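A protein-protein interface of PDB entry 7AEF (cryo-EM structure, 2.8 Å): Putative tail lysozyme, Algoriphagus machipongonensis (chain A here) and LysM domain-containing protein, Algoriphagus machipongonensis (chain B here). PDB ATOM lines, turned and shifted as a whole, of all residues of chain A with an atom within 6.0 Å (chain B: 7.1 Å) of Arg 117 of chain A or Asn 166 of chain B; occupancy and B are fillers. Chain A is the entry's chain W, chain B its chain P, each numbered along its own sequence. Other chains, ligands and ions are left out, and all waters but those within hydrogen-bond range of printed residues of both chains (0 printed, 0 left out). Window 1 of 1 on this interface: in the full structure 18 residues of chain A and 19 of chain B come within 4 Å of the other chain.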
ATOM      1  N   PHE A   8      13.568 -19.441  29.312  1.00  0.00           N
ATOM      2  CA  PHE A   8      12.706 -20.412  28.638  1.00  0.00           C
ATOM      3  C   PHE A   8      12.843 -21.813  29.198  1.00  0.00           C
ATOM      4  O   PHE A   8      12.207 -22.737  28.685  1.00  0.00           O
ATOM      5  CB  PHE A   8      12.889 -20.430  27.095  1.00  0.00           C
ATOM      6  CG  PHE A   8      14.252 -20.780  26.581  1.00  0.00           C
ATOM      7  CD1 PHE A   8      14.687 -22.094  26.481  1.00  0.00           C
ATOM      8  CD2 PHE A   8      15.053 -19.788  26.074  1.00  0.00           C
ATOM      9  CE1 PHE A   8      15.910 -22.386  25.965  1.00  0.00           C
ATOM     10  CE2 PHE A   8      16.277 -20.083  25.547  1.00  0.00           C
ATOM     11  CZ  PHE A   8      16.703 -21.383  25.497  1.00  0.00           C
ATOM     12  N   LEU A   9      13.654 -22.000  30.217  1.00  0.00           N
ATOM     13  CA  LEU A   9      13.671 -23.288  30.868  1.00  0.00           C
ATOM     14  C   LEU A   9      12.560 -23.316  31.893  1.00  0.00           C
ATOM     15  O   LEU A   9      12.006 -24.376  32.193  1.00  0.00           O
ATOM     16  CB  LEU A   9      15.051 -23.551  31.488  1.00  0.00           C
ATOM     17  CG  LEU A   9      16.273 -23.555  30.549  1.00  0.00           C
ATOM     18  CD1 LEU A   9      17.535 -23.793  31.356  1.00  0.00           C
ATOM     19  CD2 LEU A   9      16.139 -24.604  29.449  1.00  0.00           C
ATOM     20  N   LEU A  85      12.569 -38.485  24.347  1.00  0.00           N
ATOM     21  CA  LEU A  85      12.097 -37.800  23.139  1.00  0.00           C
ATOM     22  C   LEU A  85      10.636 -37.397  23.241  1.00  0.00           C
ATOM     23  O   LEU A  85      10.254 -36.313  22.789  1.00  0.00           O
ATOM     24  CB  LEU A  85      12.260 -38.682  21.914  1.00  0.00           C
ATOM     25  CG  LEU A  85      13.661 -38.958  21.405  1.00  0.00           C
ATOM     26  CD1 LEU A  85      13.589 -40.027  20.360  1.00  0.00           C
ATOM     27  CD2 LEU A  85      14.262 -37.704  20.829  1.00  0.00           C
ATOM     28  N   GLU A  88      10.635 -35.049  27.574  1.00  0.00           N
ATOM     29  CA  GLU A  88      11.482 -33.956  28.095  1.00  0.00           C
ATOM     30  C   GLU A  88      12.206 -33.152  27.003  1.00  0.00           C
ATOM     31  O   GLU A  88      13.370 -33.416  26.669  1.00  0.00           O
ATOM     32  CB  GLU A  88      12.453 -34.465  29.161  1.00  0.00           C
ATOM     33  CG  GLU A  88      13.387 -33.372  29.785  1.00  0.00           C
ATOM     34  CD  GLU A  88      12.682 -32.110  30.269  1.00  0.00           C
ATOM     35  OE1 GLU A  88      12.210 -32.075  31.413  1.00  0.00           O
ATOM     36  OE2 GLU A  88      12.619 -31.132  29.511  1.00  0.00           O
ATOM     37  N   PRO A  89      11.536 -32.102  26.490  1.00  0.00           N
ATOM     38  CA  PRO A  89      12.016 -31.252  25.372  1.00  0.00           C
ATOM     39  C   PRO A  89      13.275 -30.441  25.610  1.00  0.00           C
ATOM     40  O   PRO A  89      13.833 -29.887  24.653  1.00  0.00           O
ATOM     41  CB  PRO A  89      10.838 -30.284  25.184  1.00  0.00           C
ATOM     42  CG  PRO A  89       9.679 -30.965  25.782  1.00  0.00           C
ATOM     43  CD  PRO A  89      10.191 -31.727  26.921  1.00  0.00           C
ATOM     44  N   ARG A  90      13.697 -30.270  26.848  1.00  0.00           N
ATOM     45  CA  ARG A  90      14.821 -29.395  27.122  1.00  0.00           C
ATOM     46  C   ARG A  90      16.190 -30.067  27.030  1.00  0.00           C
ATOM     47  O   ARG A  90      17.193 -29.359  27.147  1.00  0.00           O
ATOM     48  CB  ARG A  90      14.622 -28.744  28.495  1.00  0.00           C
ATOM     49  CG  ARG A  90      13.406 -27.787  28.512  1.00  0.00           C
ATOM     50  CD  ARG A  90      13.020 -27.272  29.889  1.00  0.00           C
ATOM     51  NE  ARG A  90      12.549 -28.357  30.748  1.00  0.00           N
ATOM     52  CZ  ARG A  90      12.133 -28.246  32.009  1.00  0.00           C
ATOM     53  NH1 ARG A  90      12.086 -27.084  32.641  1.00  0.00           N
ATOM     54  NH2 ARG A  90      11.763 -29.332  32.658  1.00  0.00           N
ATOM     55  N   ILE A  91      16.304 -31.395  26.842  1.00  0.00           N
ATOM     56  CA  ILE A  91      17.635 -32.011  26.832  1.00  0.00           C
ATOM     57  C   ILE A  91      17.893 -32.933  25.646  1.00  0.00           C
ATOM     58  O   ILE A  91      16.980 -33.467  25.018  1.00  0.00           O
ATOM     59  CB  ILE A  91      17.935 -32.815  28.112  1.00  0.00           C
ATOM     60  CG1 ILE A  91      17.033 -34.051  28.209  1.00  0.00           C
ATOM     61  CG2 ILE A  91      17.808 -31.936  29.323  1.00  0.00           C
ATOM     62  CD1 ILE A  91      17.426 -35.039  29.275  1.00  0.00           C
ATOM     63  N   ASP A  92      19.187 -33.176  25.413  1.00  0.00           N
ATOM     64  CA  ASP A  92      19.727 -34.164  24.470  1.00  0.00           C
ATOM     65  C   ASP A  92      20.596 -35.169  25.215  1.00  0.00           C
ATOM     66  O   ASP A  92      21.616 -34.772  25.799  1.00  0.00           O
ATOM     67  CB  ASP A  92      20.585 -33.501  23.392  1.00  0.00           C
ATOM     68  CG  ASP A  92      19.801 -32.794  22.325  1.00  0.00           C
ATOM     69  OD1 ASP A  92      19.001 -33.427  21.632  1.00  0.00           O
ATOM     70  OD2 ASP A  92      19.986 -31.579  22.174  1.00  0.00           O
ATOM     71  N   ILE A 115      22.987 -33.387  27.976  1.00  0.00           N
ATOM     72  CA  ILE A 115      23.324 -31.994  27.680  1.00  0.00           C
ATOM     73  C   ILE A 115      22.067 -31.118  27.637  1.00  0.00           C
ATOM     74  O   ILE A 115      21.085 -31.454  26.968  1.00  0.00           O
ATOM     75  CB  ILE A 115      24.094 -31.915  26.351  1.00  0.00           C
ATOM     76  CG1 ILE A 115      25.404 -32.691  26.497  1.00  0.00           C
ATOM     77  CG2 ILE A 115      24.331 -30.470  25.931  1.00  0.00           C
ATOM     78  CD1 ILE A 115      26.124 -32.977  25.219  1.00  0.00           C
ATOM     79  N   VAL A 116      22.113 -29.973  28.317  1.00  0.00           N
ATOM     80  CA  VAL A 116      20.993 -29.033  28.328  1.00  0.00           C
ATOM     81  C   VAL A 116      21.040 -28.140  27.083  1.00  0.00           C
ATOM     82  O   VAL A 116      22.081 -27.564  26.765  1.00  0.00           O
ATOM     83  CB  VAL A 116      21.015 -28.214  29.629  1.00  0.00           C
ATOM     84  CG1 VAL A 116      19.942 -27.156  29.630  1.00  0.00           C
ATOM     85  CG2 VAL A 116      20.827 -29.149  30.812  1.00  0.00           C
ATOM     86  N   ARG A 117      19.909 -28.025  26.382  1.00  0.00           N
ATOM     87  CA  ARG A 117      19.809 -27.266  25.133  1.00  0.00           C
ATOM     88  C   ARG A 117      19.901 -25.744  25.305  1.00  0.00           C
ATOM     89  O   ARG A 117      19.252 -25.153  26.171  1.00  0.00           O
ATOM     90  CB  ARG A 117      18.488 -27.599  24.446  1.00  0.00           C
ATOM     91  CG  ARG A 117      18.459 -28.978  23.856  1.00  0.00           C
ATOM     92  CD  ARG A 117      17.120 -29.336  23.317  1.00  0.00           C
ATOM     93  NE  ARG A 117      17.216 -30.579  22.572  1.00  0.00           N
ATOM     94  CZ  ARG A 117      16.197 -31.335  22.175  1.00  0.00           C
ATOM     95  NH1 ARG A 117      14.940 -31.024  22.453  1.00  0.00           N
ATOM     96  NH2 ARG A 117      16.450 -32.427  21.483  1.00  0.00           N
ATOM     97  N   ALA A 118      20.658 -25.097  24.412  1.00  0.00           N
ATOM     98  CA  ALA A 118      20.825 -23.644  24.399  1.00  0.00           C
ATOM     99  C   ALA A 118      19.762 -22.900  23.595  1.00  0.00           C
ATOM    100  O   ALA A 118      19.770 -21.667  23.580  1.00  0.00           O
ATOM    101  CB  ALA A 118      22.189 -23.282  23.823  1.00  0.00           C
ATOM    102  N   THR A 119      18.916 -23.604  22.853  1.00  0.00           N
ATOM    103  CA  THR A 119      17.877 -23.028  22.002  1.00  0.00           C
ATOM    104  C   THR A 119      16.540 -23.620  22.424  1.00  0.00           C
ATOM    105  O   THR A 119      16.523 -24.722  22.935  1.00  0.00           O
ATOM    106  CB  THR A 119      18.169 -23.348  20.524  1.00  0.00           C
ATOM    107  OG1 THR A 119      19.448 -22.829  20.164  1.00  0.00           O
ATOM    108  CG2 THR A 119      17.150 -22.771  19.580  1.00  0.00           C
ATOM    109  N   ASN A 120      15.421 -22.922  22.210  1.00  0.00           N
ATOM    110  CA  ASN A 120      14.123 -23.349  22.709  1.00  0.00           C
ATOM    111  C   ASN A 120      13.372 -24.293  21.767  1.00  0.00           C
ATOM    112  O   ASN A 120      13.102 -23.955  20.610  1.00  0.00           O
ATOM    113  CB  ASN A 120      13.262 -22.146  23.020  1.00  0.00           C
ATOM    114  CG  ASN A 120      12.093 -22.553  23.777  1.00  0.00           C
ATOM    115  OD1 ASN A 120      12.159 -23.529  24.519  1.00  0.00           O
ATOM    116  ND2 ASN A 120      10.997 -21.876  23.588  1.00  0.00           N
ATOM    117  N   SER A 121      13.012 -25.462  22.296  1.00  0.00           N
ATOM    118  CA  SER A 121      12.268 -26.501  21.591  1.00  0.00           C
ATOM    119  C   SER A 121      10.812 -26.132  21.335  1.00  0.00           C
ATOM    120  O   SER A 121      10.160 -25.480  22.148  1.00  0.00           O
ATOM    121  CB  SER A 121      12.270 -27.786  22.400  1.00  0.00           C
ATOM    122  OG  SER A 121      11.379 -28.701  21.810  1.00  0.00           O
ATOM    123  N   ARG A 122      10.272 -26.660  20.232  1.00  0.00           N
ATOM    124  CA  ARG A 122       8.886 -26.423  19.816  1.00  0.00           C
ATOM    125  C   ARG A 122       7.860 -27.151  20.670  1.00  0.00           C
ATOM    126  O   ARG A 122       6.655 -26.975  20.459  1.00  0.00           O
ATOM    127  CB  ARG A 122       8.693 -26.868  18.377  1.00  0.00           C
ATOM    128  CG  ARG A 122       9.429 -26.061  17.348  1.00  0.00           C
ATOM    129  CD  ARG A 122       9.179 -26.604  15.970  1.00  0.00           C
ATOM    130  NE  ARG A 122       9.981 -25.934  14.952  1.00  0.00           N
ATOM    131  CZ  ARG A 122       9.640 -24.817  14.309  1.00  0.00           C
ATOM    132  NH1 ARG A 122       8.501 -24.197  14.566  1.00  0.00           N
ATOM    133  NH2 ARG A 122      10.453 -24.312  13.399  1.00  0.00           N
ATOM    134  N   ARG B 161       8.857 -38.363  14.528  1.00  0.00           N
ATOM    135  CA  ARG B 161       9.706 -37.816  13.472  1.00  0.00           C
ATOM    136  C   ARG B 161      10.074 -36.364  13.754  1.00  0.00           C
ATOM    137  O   ARG B 161      11.228 -35.962  13.569  1.00  0.00           O
ATOM    138  CB  ARG B 161       9.017 -37.937  12.112  1.00  0.00           C
ATOM    139  CG  ARG B 161       9.866 -37.385  10.971  1.00  0.00           C
ATOM    140  CD  ARG B 161       9.172 -37.385   9.641  1.00  0.00           C
ATOM    141  NE  ARG B 161       7.898 -36.678   9.658  1.00  0.00           N
ATOM    142  CZ  ARG B 161       7.760 -35.371   9.462  1.00  0.00           C
ATOM    143  NH1 ARG B 161       8.824 -34.615   9.251  1.00  0.00           N
ATOM    144  NH2 ARG B 161       6.558 -34.821   9.485  1.00  0.00           N
ATOM    145  N   THR B 162       9.110 -35.570  14.213  1.00  0.00           N
ATOM    146  CA  THR B 162       9.381 -34.184  14.566  1.00  0.00           C
ATOM    147  C   THR B 162      10.219 -34.046  15.830  1.00  0.00           C
ATOM    148  O   THR B 162      10.891 -33.027  15.996  1.00  0.00           O
ATOM    149  CB  THR B 162       8.073 -33.410  14.731  1.00  0.00           C
ATOM    150  OG1 THR B 162       7.238 -34.070  15.685  1.00  0.00           O
ATOM    151  CG2 THR B 162       7.337 -33.318  13.412  1.00  0.00           C
ATOM    152  N   ALA B 163      10.204 -35.035  16.722  1.00  0.00           N
ATOM    153  CA  ALA B 163      11.067 -34.975  17.895  1.00  0.00           C
ATOM    154  C   ALA B 163      12.500 -35.369  17.563  1.00  0.00           C
ATOM    155  O   ALA B 163      13.435 -34.930  18.238  1.00  0.00           O
ATOM    156  CB  ALA B 163      10.509 -35.870  18.997  1.00  0.00           C
ATOM    157  N   GLN B 164      12.693 -36.194  16.535  1.00  0.00           N
ATOM    158  CA  GLN B 164      14.039 -36.560  16.106  1.00  0.00           C
ATOM    159  C   GLN B 164      14.638 -35.499  15.194  1.00  0.00           C
ATOM    160  O   GLN B 164      15.848 -35.261  15.228  1.00  0.00           O
ATOM    161  CB  GLN B 164      14.016 -37.920  15.411  1.00  0.00           C
ATOM    162  CG  GLN B 164      13.849 -39.090  16.353  1.00  0.00           C
ATOM    163  CD  GLN B 164      13.517 -40.385  15.641  1.00  0.00           C
ATOM    164  OE1 GLN B 164      12.717 -40.413  14.713  1.00  0.00           O
ATOM    165  NE2 GLN B 164      14.137 -41.469  16.079  1.00  0.00           N
ATOM    166  N   GLU B 165      13.810 -34.868  14.366  1.00  0.00           N
ATOM    167  CA  GLU B 165      14.197 -33.684  13.602  1.00  0.00           C
ATOM    168  C   GLU B 165      13.887 -32.462  14.454  1.00  0.00           C
ATOM    169  O   GLU B 165      12.863 -31.793  14.291  1.00  0.00           O
ATOM    170  CB  GLU B 165      13.444 -33.614  12.283  1.00  0.00           C
ATOM    171  CG  GLU B 165      13.678 -34.760  11.349  1.00  0.00           C
ATOM    172  CD  GLU B 165      12.732 -34.742  10.171  1.00  0.00           C
ATOM    173  OE1 GLU B 165      11.888 -33.826  10.088  1.00  0.00           O
ATOM    174  OE2 GLU B 165      12.830 -35.653   9.321  1.00  0.00           O
ATOM    175  N   ASN B 166      14.785 -32.164  15.387  1.00  0.00           N
ATOM    176  CA  ASN B 166      14.602 -31.028  16.287  1.00  0.00           C
ATOM    177  C   ASN B 166      14.877 -29.756  15.485  1.00  0.00           C
ATOM    178  O   ASN B 166      15.964 -29.173  15.516  1.00  0.00           O
ATOM    179  CB  ASN B 166      15.503 -31.179  17.509  1.00  0.00           C
ATOM    180  CG  ASN B 166      15.440 -29.997  18.439  1.00  0.00           C
ATOM    181  OD1 ASN B 166      14.385 -29.413  18.661  1.00  0.00           O
ATOM    182  ND2 ASN B 166      16.585 -29.629  18.985  1.00  0.00           N
ATOM    183  N   ASN B 167      13.864 -29.334  14.730  1.00  0.00           N
ATOM    184  CA  ASN B 167      14.008 -28.260  13.757  1.00  0.00           C
ATOM    185  C   ASN B 167      14.044 -26.917  14.468  1.00  0.00           C
ATOM    186  O   ASN B 167      13.100 -26.554  15.175  1.00  0.00           O
ATOM    187  CB  ASN B 167      12.864 -28.309  12.751  1.00  0.00           C
ATOM    188  CG  ASN B 167      13.125 -29.282  11.630  1.00  0.00           C
ATOM    189  OD1 ASN B 167      14.240 -29.392  11.137  1.00  0.00           O
ATOM    190  ND2 ASN B 167      12.099 -30.009  11.232  1.00  0.00           N
ATOM    191  N   GLN B 168      15.129 -26.178  14.286  1.00  0.00           N
ATOM    192  CA  GLN B 168      15.263 -24.883  14.929  1.00  0.00           C
ATOM    193  C   GLN B 168      15.514 -23.778  13.910  1.00  0.00           C
ATOM    194  O   GLN B 168      14.572 -23.174  13.394  1.00  0.00           O
ATOM    195  CB  GLN B 168      16.385 -24.921  15.959  1.00  0.00           C
ATOM    196  CG  GLN B 168      17.766 -24.745  15.384  1.00  0.00           C
ATOM    197  CD  GLN B 168      18.824 -25.363  16.261  1.00  0.00           C
ATOM    198  OE1 GLN B 168      18.636 -26.450  16.805  1.00  0.00           O
ATOM    199  NE2 GLN B 168      19.947 -24.674  16.407  1.00  0.00           N
ATOM    200  N   TYR B 175      20.484 -18.002  23.604  1.00  0.00           N
ATOM    201  CA  TYR B 175      21.322 -17.235  24.518  1.00  0.00           C
ATOM    202  C   TYR B 175      22.777 -17.676  24.392  1.00  0.00           C
ATOM    203  O   TYR B 175      23.067 -18.844  24.137  1.00  0.00           O
ATOM    204  CB  TYR B 175      20.836 -17.343  25.993  1.00  0.00           C
ATOM    205  CG  TYR B 175      20.793 -18.731  26.603  1.00  0.00           C
ATOM    206  CD1 TYR B 175      21.921 -19.292  27.195  1.00  0.00           C
ATOM    207  CD2 TYR B 175      19.618 -19.462  26.628  1.00  0.00           C
ATOM    208  CE1 TYR B 175      21.887 -20.548  27.748  1.00  0.00           C
ATOM    209  CE2 TYR B 175      19.574 -20.725  27.187  1.00  0.00           C
ATOM    210  CZ  TYR B 175      20.712 -21.261  27.741  1.00  0.00           C
ATOM    211  OH  TYR B 175      20.677 -22.513  28.303  1.00  0.00           O
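The guanidinium group of Arg 122 of chain A sits at hydrogen-bond distance from the backbone carbonyl oxygen of Asn 167 of chain B, at 3.2 Å.
The guanidinium group (NH2) of Arg 117 of chain A lies within salt-bridge range of the side-chain carboxylate (OD1) of Asp 92 of chain A (2.7 Å).
The backbone carbonyl oxygen (O) of Pro 89 of chain A lies within hydrogen-bond range of the guanidinium group (NH1) of Arg 117 of chain A.
The backbone carbonyl oxygen (O) of Arg 90 of chain A lies within hydrogen-bond range of the backbone NH (N) of Arg 117 of chain A (3.1 Å).
Among the printed residues, pairs that only touch across the chains: Phe 8 of chain A with Tyr 175 of chain B (3.4 Å), Leu 85 of chain A with Ala 163 of chain B (3.8 Å), Arg 117 of chain A with Asn 166 of chain B (3.6 Å), Arg 117 of chain A with Tyr 175 of chain B (3.7 Å) and Ala 118 of chain A with Tyr 175 of chain B (3.7 Å).
Of the printed residues of chain B, Arg 117 of chain A touches Asn 166 and Tyr 175.
Asn 166 of chain B touches one residue of chain A.
Printed residues of chain B within 4 Å of Phe 8 of chain A: Tyr 175.
Of the printed residues of chain B, Leu 85 of chain A touches Ala 163 (3.8 Å).
Printed residues of chain B within 4 Å of Arg 122 of chain A: Asn 167.
Of the printed residues of chain A, Asn 167 of chain B touches Arg 122.
Thr 162 of chain B touches none of the printed residues of chain A.
The nearest residue of chain B that does not touch Arg 117 of chain A is Ala 163 of chain B (5.1 Å).
The nearest printed residue of chain B that does not touch Leu 85 of chain A is Gln 164 of chain B (4.1 Å).
Printed residues of chain A that touch a printed residue of chain B: Phe 8, Leu 85, Arg 117, Ala 118 and Arg 122.
Hydrophobic or aromatic side chains of chain A that line the printed part of chain B: Phe 8 and Leu 85.
Printed residues of chain B that touch a printed residue of chain A: Ala 163, Asn 166, Asn 167 and Tyr 175.
Hydrophobic or aromatic side chains of chain B that line the printed part of chain A: Ala 163 and Tyr 175.
Among the printed residues, 6 pairs touch across the chains.
Among the printed residues, no Asp or Glu carboxylate lies within 4 Å of a Lys or Arg side-chain nitrogen of the other chain.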
